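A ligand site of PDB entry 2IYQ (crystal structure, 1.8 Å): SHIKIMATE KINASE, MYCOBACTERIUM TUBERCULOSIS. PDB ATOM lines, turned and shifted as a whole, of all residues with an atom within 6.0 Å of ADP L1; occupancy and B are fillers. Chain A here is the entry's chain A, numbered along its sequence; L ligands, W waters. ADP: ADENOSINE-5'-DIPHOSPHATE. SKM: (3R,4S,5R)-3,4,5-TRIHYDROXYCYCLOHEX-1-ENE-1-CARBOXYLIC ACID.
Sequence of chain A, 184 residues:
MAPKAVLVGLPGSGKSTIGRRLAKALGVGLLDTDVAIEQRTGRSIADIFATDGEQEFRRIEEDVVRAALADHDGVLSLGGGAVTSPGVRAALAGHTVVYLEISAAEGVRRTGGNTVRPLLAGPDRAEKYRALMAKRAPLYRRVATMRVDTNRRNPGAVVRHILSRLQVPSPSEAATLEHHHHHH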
ATOM      1  N   GLY A   9      -0.649  34.183 -12.486  1.00  0.00           N
ATOM      2  CA  GLY A   9       0.695  33.797 -12.867  1.00  0.00           C
ATOM      3  C   GLY A   9       0.664  32.645 -13.828  1.00  0.00           C
ATOM      4  O   GLY A   9      -0.410  32.125 -14.234  1.00  0.00           O
ATOM      5  N   LEU A  10       1.853  32.263 -14.276  1.00  0.00           N
ATOM      6  CA  LEU A  10       1.979  31.260 -15.308  1.00  0.00           C
ATOM      7  C   LEU A  10       1.511  29.901 -14.822  1.00  0.00           C
ATOM      8  O   LEU A  10       1.483  29.660 -13.594  1.00  0.00           O
ATOM      9  CB  LEU A  10       3.450  31.110 -15.728  1.00  0.00           C
ATOM     10  CG  LEU A  10       4.041  32.195 -16.613  1.00  0.00           C
ATOM     11  CD1 LEU A  10       5.545  32.140 -16.687  1.00  0.00           C
ATOM     12  CD2 LEU A  10       3.461  32.126 -18.006  1.00  0.00           C
ATOM     13  N   PRO A  11       1.168  28.998 -15.743  1.00  0.00           N
ATOM     14  CA  PRO A  11       1.001  27.596 -15.339  1.00  0.00           C
ATOM     15  C   PRO A  11       2.167  27.099 -14.529  1.00  0.00           C
ATOM     16  O   PRO A  11       3.293  27.395 -14.862  1.00  0.00           O
ATOM     17  CB  PRO A  11       0.953  26.838 -16.672  1.00  0.00           C
ATOM     18  CG  PRO A  11       1.320  27.830 -17.719  1.00  0.00           C
ATOM     19  CD  PRO A  11       0.981  29.163 -17.208  1.00  0.00           C
ATOM     20  N   GLY A  12       1.895  26.421 -13.412  1.00  0.00           N
ATOM     21  CA  GLY A  12       2.979  25.980 -12.456  1.00  0.00           C
ATOM     22  C   GLY A  12       3.536  26.989 -11.496  1.00  0.00           C
ATOM     23  O   GLY A  12       4.437  26.651 -10.732  1.00  0.00           O
ATOM     24  N   SER A  13       3.068  28.258 -11.518  1.00  0.00           N
ATOM     25  CA  SER A  13       3.543  29.222 -10.542  1.00  0.00           C
ATOM     26  C   SER A  13       2.995  28.924  -9.128  1.00  0.00           C
ATOM     27  O   SER A  13       3.505  29.469  -8.172  1.00  0.00           O
ATOM     28  CB  SER A  13       3.203  30.658 -10.944  1.00  0.00           C
ATOM     29  OG  SER A  13       1.802  30.744 -11.206  1.00  0.00           O
ATOM     30  N   GLY A  14       1.927  28.131  -9.040  1.00  0.00           N
ATOM     31  CA  GLY A  14       1.380  27.733  -7.769  1.00  0.00           C
ATOM     32  C   GLY A  14       0.024  28.296  -7.462  1.00  0.00           C
ATOM     33  O   GLY A  14      -0.399  28.296  -6.333  1.00  0.00           O
ATOM     34  N   LYS A  15      -0.748  28.703  -8.449  1.00  0.00           N
ATOM     35  CA  LYS A  15      -2.091  29.301  -8.116  1.00  0.00           C
ATOM     36  C   LYS A  15      -3.021  28.361  -7.344  1.00  0.00           C
ATOM     37  O   LYS A  15      -3.680  28.770  -6.362  1.00  0.00           O
ATOM     38  CB  LYS A  15      -2.803  29.796  -9.388  1.00  0.00           C
ATOM     39  CG  LYS A  15      -1.930  30.835 -10.087  1.00  0.00           C
ATOM     40  CD  LYS A  15      -2.637  31.321 -11.396  1.00  0.00           C
ATOM     41  CE  LYS A  15      -2.735  30.226 -12.439  1.00  0.00           C
ATOM     42  NZ  LYS A  15      -1.452  29.722 -12.971  1.00  0.00           N
ATOM     43  N   SER A  16      -3.126  27.146  -7.805  1.00  0.00           N
ATOM     44  CA  SER A  16      -4.032  26.202  -7.188  1.00  0.00           C
ATOM     45  C   SER A  16      -3.558  25.834  -5.797  1.00  0.00           C
ATOM     46  O   SER A  16      -4.353  25.709  -4.842  1.00  0.00           O
ATOM     47  CB  SER A  16      -4.121  24.969  -8.076  1.00  0.00           C
ATOM     48  OG  SER A  16      -4.813  25.300  -9.230  1.00  0.00           O
ATOM     49  N   THR A  17      -2.238  25.715  -5.676  1.00  0.00           N
ATOM     50  CA  THR A  17      -1.571  25.235  -4.472  1.00  0.00           C
ATOM     51  C   THR A  17      -1.530  26.276  -3.382  1.00  0.00           C
ATOM     52  O   THR A  17      -1.959  26.027  -2.251  1.00  0.00           O
ATOM     53  CB  THR A  17      -0.125  24.739  -4.813  1.00  0.00           C
ATOM     54  OG1 THR A  17      -0.223  23.666  -5.762  1.00  0.00           O
ATOM     55  CG2 THR A  17       0.619  24.289  -3.577  1.00  0.00           C
ATOM     56  N   ILE A  18      -1.012  27.459  -3.712  1.00  0.00           N
ATOM     57  CA  ILE A  18      -0.973  28.604  -2.829  1.00  0.00           C
ATOM     58  C   ILE A  18      -2.431  28.992  -2.518  1.00  0.00           C
ATOM     59  O   ILE A  18      -2.714  29.300  -1.393  1.00  0.00           O
ATOM     60  CB  ILE A  18      -0.209  29.755  -3.468  1.00  0.00           C
ATOM     61  CG1 ILE A  18       1.223  29.322  -3.842  1.00  0.00           C
ATOM     62  CG2 ILE A  18      -0.183  31.002  -2.636  1.00  0.00           C
ATOM     63  CD1 ILE A  18       2.079  28.780  -2.657  1.00  0.00           C
ATOM     64  N   ASP A  32     -11.343  28.172  -7.589  1.00  0.00           N
ATOM     65  CA  ASP A  32     -10.375  28.022  -8.681  1.00  0.00           C
ATOM     66  C   ASP A  32     -11.149  28.067  -9.980  1.00  0.00           C
ATOM     67  O   ASP A  32     -11.951  27.227 -10.264  1.00  0.00           O
ATOM     68  CB  ASP A  32      -9.644  26.689  -8.511  1.00  0.00           C
ATOM     69  CG  ASP A  32      -8.476  26.506  -9.461  1.00  0.00           C
ATOM     70  OD1 ASP A  32      -8.447  27.158 -10.537  1.00  0.00           O
ATOM     71  OD2 ASP A  32      -7.590  25.687  -9.128  1.00  0.00           O
ATOM     72  N   LEU A 100       2.146  35.512  -8.745  1.00  0.00           N
ATOM     73  CA  LEU A 100       3.128  34.486  -8.345  1.00  0.00           C
ATOM     74  C   LEU A 100       4.136  34.353  -9.481  1.00  0.00           C
ATOM     75  O   LEU A 100       3.825  33.926 -10.570  1.00  0.00           O
ATOM     76  CB  LEU A 100       2.458  33.161  -8.079  1.00  0.00           C
ATOM     77  CG  LEU A 100       1.340  33.086  -7.008  1.00  0.00           C
ATOM     78  CD1 LEU A 100       0.716  31.718  -6.975  1.00  0.00           C
ATOM     79  CD2 LEU A 100       1.845  33.470  -5.686  1.00  0.00           C
ATOM     80  N   GLU A 106      12.327  26.579 -13.654  1.00  0.00           N
ATOM     81  CA  GLU A 106      11.585  25.962 -12.558  1.00  0.00           C
ATOM     82  C   GLU A 106      10.161  25.697 -12.964  1.00  0.00           C
ATOM     83  O   GLU A 106       9.582  24.652 -12.631  1.00  0.00           O
ATOM     84  CB  GLU A 106      11.709  26.825 -11.294  1.00  0.00           C
ATOM     85  CG  GLU A 106      11.054  26.192  -9.997  1.00  0.00           C
ATOM     86  CD  GLU A 106      11.482  24.743  -9.650  1.00  0.00           C
ATOM     87  OE1 GLU A 106      12.613  24.353  -9.956  1.00  0.00           O
ATOM     88  OE2 GLU A 106      10.678  24.012  -9.055  1.00  0.00           O
ATOM     89  N   ARG A 110       8.158  22.223 -12.720  1.00  0.00           N
ATOM     90  CA  ARG A 110       6.915  22.035 -11.943  1.00  0.00           C
ATOM     91  C   ARG A 110       5.775  21.433 -12.719  1.00  0.00           C
ATOM     92  O   ARG A 110       4.918  20.750 -12.127  1.00  0.00           O
ATOM     93  CB  ARG A 110       6.443  23.345 -11.342  1.00  0.00           C
ATOM     94  CG  ARG A 110       7.297  23.738 -10.172  1.00  0.00           C
ATOM     95  CD  ARG A 110       6.718  24.948  -9.477  1.00  0.00           C
ATOM     96  NE  ARG A 110       7.656  25.530  -8.561  1.00  0.00           N
ATOM     97  CZ  ARG A 110       7.479  26.686  -7.916  1.00  0.00           C
ATOM     98  NH1 ARG A 110       6.360  27.400  -8.127  1.00  0.00           N
ATOM     99  NH2 ARG A 110       8.375  27.144  -7.115  1.00  0.00           N
ATOM    100  N   THR A 111       5.728  21.721 -14.016  1.00  0.00           N
ATOM    101  CA  THR A 111       4.635  21.282 -14.874  1.00  0.00           C
ATOM    102  C   THR A 111       4.980  19.984 -15.639  1.00  0.00           C
ATOM    103  O   THR A 111       4.157  19.498 -16.413  1.00  0.00           O
ATOM    104  CB  THR A 111       4.268  22.367 -15.877  1.00  0.00           C
ATOM    105  OG1 THR A 111       5.397  22.710 -16.699  1.00  0.00           O
ATOM    106  CG2 THR A 111       3.830  23.637 -15.161  1.00  0.00           C
ATOM    107  N   ARG A 117      -2.778  20.519 -19.462  1.00  0.00           N
ATOM    108  CA  ARG A 117      -2.651  21.885 -20.008  1.00  0.00           C
ATOM    109  C   ARG A 117      -2.385  21.905 -21.546  1.00  0.00           C
ATOM    110  O   ARG A 117      -1.236  21.718 -21.985  1.00  0.00           O
ATOM    111  CB  ARG A 117      -1.547  22.647 -19.260  1.00  0.00           C
ATOM    112  CG  ARG A 117      -1.832  22.812 -17.746  1.00  0.00           C
ATOM    113  CD  ARG A 117      -0.888  23.832 -17.111  1.00  0.00           C
ATOM    114  NE  ARG A 117      -0.801  23.863 -15.621  1.00  0.00           N
ATOM    115  CZ  ARG A 117      -0.049  23.065 -14.845  1.00  0.00           C
ATOM    116  NH1 ARG A 117       0.669  22.051 -15.366  1.00  0.00           N
ATOM    117  NH2 ARG A 117      -0.040  23.257 -13.516  1.00  0.00           N
ATOM    118  N   THR A 150       8.425  33.161  -6.257  1.00  0.00           N
ATOM    119  CA  THR A 150       8.243  31.824  -5.736  1.00  0.00           C
ATOM    120  C   THR A 150       9.402  30.843  -6.012  1.00  0.00           C
ATOM    121  O   THR A 150       9.301  29.678  -5.619  1.00  0.00           O
ATOM    122  CB  THR A 150       6.984  31.123  -6.219  1.00  0.00           C
ATOM    123  OG1 THR A 150       7.106  30.655  -7.575  1.00  0.00           O
ATOM    124  CG2 THR A 150       5.716  32.009  -6.035  1.00  0.00           C
ATOM    125  N   ARG A 153      11.232  29.787  -2.661  1.00  0.00           N
ATOM    126  CA  ARG A 153      10.352  29.808  -1.505  1.00  0.00           C
ATOM    127  C   ARG A 153       9.513  28.582  -1.551  1.00  0.00           C
ATOM    128  O   ARG A 153       8.951  28.260  -2.554  1.00  0.00           O
ATOM    129  CB  ARG A 153       9.413  31.050  -1.520  1.00  0.00           C
ATOM    130  CG  ARG A 153       9.972  32.293  -0.919  1.00  0.00           C
ATOM    131  CD  ARG A 153       8.871  33.357  -0.809  1.00  0.00           C
ATOM    132  NE  ARG A 153       9.397  34.588  -0.221  1.00  0.00           N
ATOM    133  CZ  ARG A 153       9.674  35.712  -0.868  1.00  0.00           C
ATOM    134  NH1 ARG A 153       9.446  35.844  -2.176  1.00  0.00           N
ATOM    135  NH2 ARG A 153      10.162  36.741  -0.213  1.00  0.00           N
ATOM    136  N   ASN A 154       9.409  27.900  -0.429  1.00  0.00           N
ATOM    137  CA  ASN A 154       8.493  26.796  -0.390  1.00  0.00           C
ATOM    138  C   ASN A 154       7.034  27.323  -0.197  1.00  0.00           C
ATOM    139  O   ASN A 154       6.836  28.469   0.131  1.00  0.00           O
ATOM    140  CB  ASN A 154       8.906  25.802   0.690  1.00  0.00           C
ATOM    141  CG  ASN A 154       8.960  26.431   2.049  1.00  0.00           C
ATOM    142  OD1 ASN A 154       8.081  27.214   2.407  1.00  0.00           O
ATOM    143  ND2 ASN A 154       9.986  26.091   2.834  1.00  0.00           N
ATOM    144  N   PRO A 155       6.041  26.491  -0.495  1.00  0.00           N
ATOM    145  CA  PRO A 155       4.684  27.021  -0.533  1.00  0.00           C
ATOM    146  C   PRO A 155       4.228  27.660   0.761  1.00  0.00           C
ATOM    147  O   PRO A 155       3.489  28.613   0.734  1.00  0.00           O
ATOM    148  CB  PRO A 155       3.815  25.811  -0.874  1.00  0.00           C
ATOM    149  CG  PRO A 155       4.758  24.824  -1.439  1.00  0.00           C
ATOM    150  CD  PRO A 155       6.043  25.046  -0.789  1.00  0.00           C
ATOM    151  N   VAL A 158       5.585  31.071   0.882  1.00  0.00           N
ATOM    152  CA  VAL A 158       4.853  31.987  -0.040  1.00  0.00           C
ATOM    153  C   VAL A 158       3.591  32.475   0.658  1.00  0.00           C
ATOM    154  O   VAL A 158       3.336  33.683   0.669  1.00  0.00           O
ATOM    155  CB  VAL A 158       4.573  31.289  -1.396  1.00  0.00           C
ATOM    156  CG1 VAL A 158       3.642  32.120  -2.247  1.00  0.00           C
ATOM    157  CG2 VAL A 158       5.909  30.973  -2.122  1.00  0.00           C
HETATM  158  PB  ADP L   1      -0.851  26.529 -11.129  1.00  0.00           P
HETATM  159  O1B ADP L   1      -2.210  26.382 -10.519  1.00  0.00           O
HETATM  160  O2B ADP L   1      -0.834  25.865 -12.490  1.00  0.00           O
HETATM  161  O3B ADP L   1      -0.188  27.918 -11.148  1.00  0.00           O
HETATM  162  PA  ADP L   1      -0.155  24.394  -9.268  1.00  0.00           P
HETATM  163  O1A ADP L   1      -1.101  23.378  -9.832  1.00  0.00           O
HETATM  164  O2A ADP L   1      -0.572  24.916  -7.935  1.00  0.00           O
HETATM  165  O3A ADP L   1       0.194  25.630 -10.248  1.00  0.00           O
HETATM  166  O5' ADP L   1       1.342  23.889  -8.891  1.00  0.00           O
HETATM  167  C5' ADP L   1       2.072  23.118  -9.871  1.00  0.00           C
HETATM  168  C4' ADP L   1       3.010  22.132  -9.145  1.00  0.00           C
HETATM  169  O4' ADP L   1       3.982  22.936  -8.566  1.00  0.00           O
HETATM  170  C3' ADP L   1       2.329  21.328  -8.042  1.00  0.00           C
HETATM  171  O3' ADP L   1       2.847  19.974  -7.834  1.00  0.00           O
HETATM  172  C2' ADP L   1       2.694  22.051  -6.825  1.00  0.00           C
HETATM  173  O2' ADP L   1       2.905  21.122  -5.771  1.00  0.00           O
HETATM  174  C1' ADP L   1       4.031  22.696  -7.200  1.00  0.00           C
HETATM  175  N9  ADP L   1       4.350  23.932  -6.535  1.00  0.00           N
HETATM  176  C8  ADP L   1       3.589  25.056  -6.553  1.00  0.00           C
HETATM  177  N7  ADP L   1       4.199  25.981  -5.828  1.00  0.00           N
HETATM  178  C5  ADP L   1       5.378  25.506  -5.378  1.00  0.00           C
HETATM  179  C6  ADP L   1       6.421  26.045  -4.561  1.00  0.00           C
HETATM  180  N6  ADP L   1       6.416  27.285  -4.104  1.00  0.00           N
HETATM  181  N1  ADP L   1       7.519  25.233  -4.245  1.00  0.00           N
HETATM  182  C2  ADP L   1       7.490  23.962  -4.751  1.00  0.00           C
HETATM  183  N3  ADP L   1       6.556  23.402  -5.507  1.00  0.00           N
HETATM  184  C4  ADP L   1       5.467  24.161  -5.833  1.00  0.00           C
HETATM  185  O12 SKM L   2      -6.785  27.731 -17.597  1.00  0.00           O
HETATM  186  C8  SKM L   2      -5.988  26.557 -17.729  1.00  0.00           C
HETATM  187  C6  SKM L   2      -5.882  26.266 -19.223  1.00  0.00           C
HETATM  188  O7  SKM L   2      -5.186  25.032 -19.471  1.00  0.00           O
HETATM  189  C5  SKM L   2      -5.204  27.435 -19.928  1.00  0.00           C
HETATM  190  C4  SKM L   2      -3.964  27.948 -19.247  1.00  0.00           C
HETATM  191  C1  SKM L   2      -3.123  28.919 -19.912  1.00  0.00           C
HETATM  192  O2  SKM L   2      -1.930  29.127 -19.559  1.00  0.00           O
HETATM  193  O3  SKM L   2      -3.657  29.625 -20.798  1.00  0.00           O
HETATM  194  C10 SKM L   2      -3.674  27.587 -17.970  1.00  0.00           C
HETATM  195  C9  SKM L   2      -4.573  26.726 -17.132  1.00  0.00           C
HETATM  196  O11 SKM L   2      -4.646  27.326 -15.825  1.00  0.00           O
HETATM  197  O   HOH W   1       3.975  22.164  -3.285  1.00  0.00           O
HETATM  198  O   HOH W   2       4.246  28.814  -5.338  1.00  0.00           O
HETATM  199  O   HOH W   3      -2.285  27.455 -14.558  1.00  0.00           O
HETATM  200  O   HOH W   4      -3.317  23.768 -11.492  1.00  0.00           O
HETATM  201  O   HOH W   5      -2.511  21.809  -8.313  1.00  0.00           O
HETATM  202  O   HOH W   6      -4.725  26.466 -12.201  1.00  0.00           O
HETATM  203  O   HOH W   7      10.128  25.928  -3.971  1.00  0.00           O
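The backbone carbonyl oxygen (O) of Leu 10 lies close to an oxygen (O3B) of ADP L1 (3.4 Å).
Residues that only touch ADP L1: Pro 155, Pro 11 and Asn 154.
Hydrophobic or aromatic side chains that line ADP L1: Pro 155.
13 residues have an atom within 4 Å of ADP L1: Leu 10, Pro 11, Gly 12, Ser 13, Gly 14, Lys 15, Ser 16, Thr 17, Arg 110, Arg 117, Arg 153, Asn 154 and Pro 155.
The nearest printed residue that does not touch ADP L1 is Thr 150 (4.04 Å).
NZ of Lys 15 is in hydrogen-bond range of O of Leu 10 (3.0 Å).
NZ of Lys 15 lies within hydrogen-bond range of O of Gly 9 (2.9 Å).
O of Gly 12 sits close to NH1 of Arg 110.
OG of Ser 16 lies within hydrogen-bond range of OD2 of Asp 32, 2.8 Å away.
The backbone carbonyl oxygen (O) of Leu 10 lies within hydrogen-bond range of the side-chain hydroxyl (OG) of Ser 13, 2.6 Å away.
The backbone carbonyl oxygen (O) of Thr 150 sits at hydrogen-bond distance from the guanidinium group (NH2) of Arg 110 (3.1 Å).
NE of Arg 110 is in salt-bridge range of OE2 of Glu 106 (3.4 Å).
Water W7 bridges N1 of ADP L1 (2.7 Å) and O of Arg 153 (3.0 Å).
Water W4 bridges an oxygen (O1A) of ADP L1 and the side-chain hydroxyl (OG) of Ser 16.
Water W2 bridges N7 of ADP L1 (2.9 Å) and O of Ser 13 (3.0 Å).
Water W3 lies within hydrogen-bond range of an oxygen (O11) of SKM L2, the side-chain amino group (NZ) of Lys 15 and an oxygen (O2B) of ADP L1.
Water W6 bridges an oxygen (O1B) of ADP L1 (3.0 Å) and the side-chain hydroxyl (OG) of Ser 16 (3.2 Å).
The backbone NH of Thr 17 sits at hydrogen-bond distance from an oxygen (O2A) of ADP L1 (2.9 Å).
The side-chain hydroxyl (OG1) of Thr 17 sits at hydrogen-bond distance from an oxygen (O2A) of ADP L1, 2.5 Å away.
N of Lys 15 is in hydrogen-bond range of O3B of ADP L1, 2.9 Å away.
O3B of ADP L1 lies within salt-bridge range of NZ of Lys 15, 2.9 Å away.
O2B of ADP L1 lies within salt-bridge range of NH2 of Arg 117, 2.9 Å away.
N of Gly 12 is in hydrogen-bond range of O2B of ADP L1 (2.9 Å).
An oxygen (O1B) of ADP L1 lies within hydrogen-bond range of the backbone NH (N) of Ser 16 (3.0 Å).
An oxygen (O1B) of ADP L1 lies within hydrogen-bond range of the side-chain hydroxyl of Ser 16 (3.1 Å).
The backbone NH (N) of Gly 14 sits at hydrogen-bond distance from an oxygen (O3B) of ADP L1, at 3.0 Å.
A nitrogen (N6) of ADP L1 sits at hydrogen-bond distance from the backbone carbonyl oxygen (O) of Arg 153 (3.1 Å).
O3B of ADP L1 is in hydrogen-bond range of N of Ser 13 (3.3 Å).
The side-chain hydroxyl of Ser 13 lies within hydrogen-bond range of an oxygen (O3B) of ADP L1, 3.5 Å away.
A nitrogen (N7) of ADP L1 lies within hydrogen-bond range of the guanidinium group of Arg 110 (3.5 Å).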
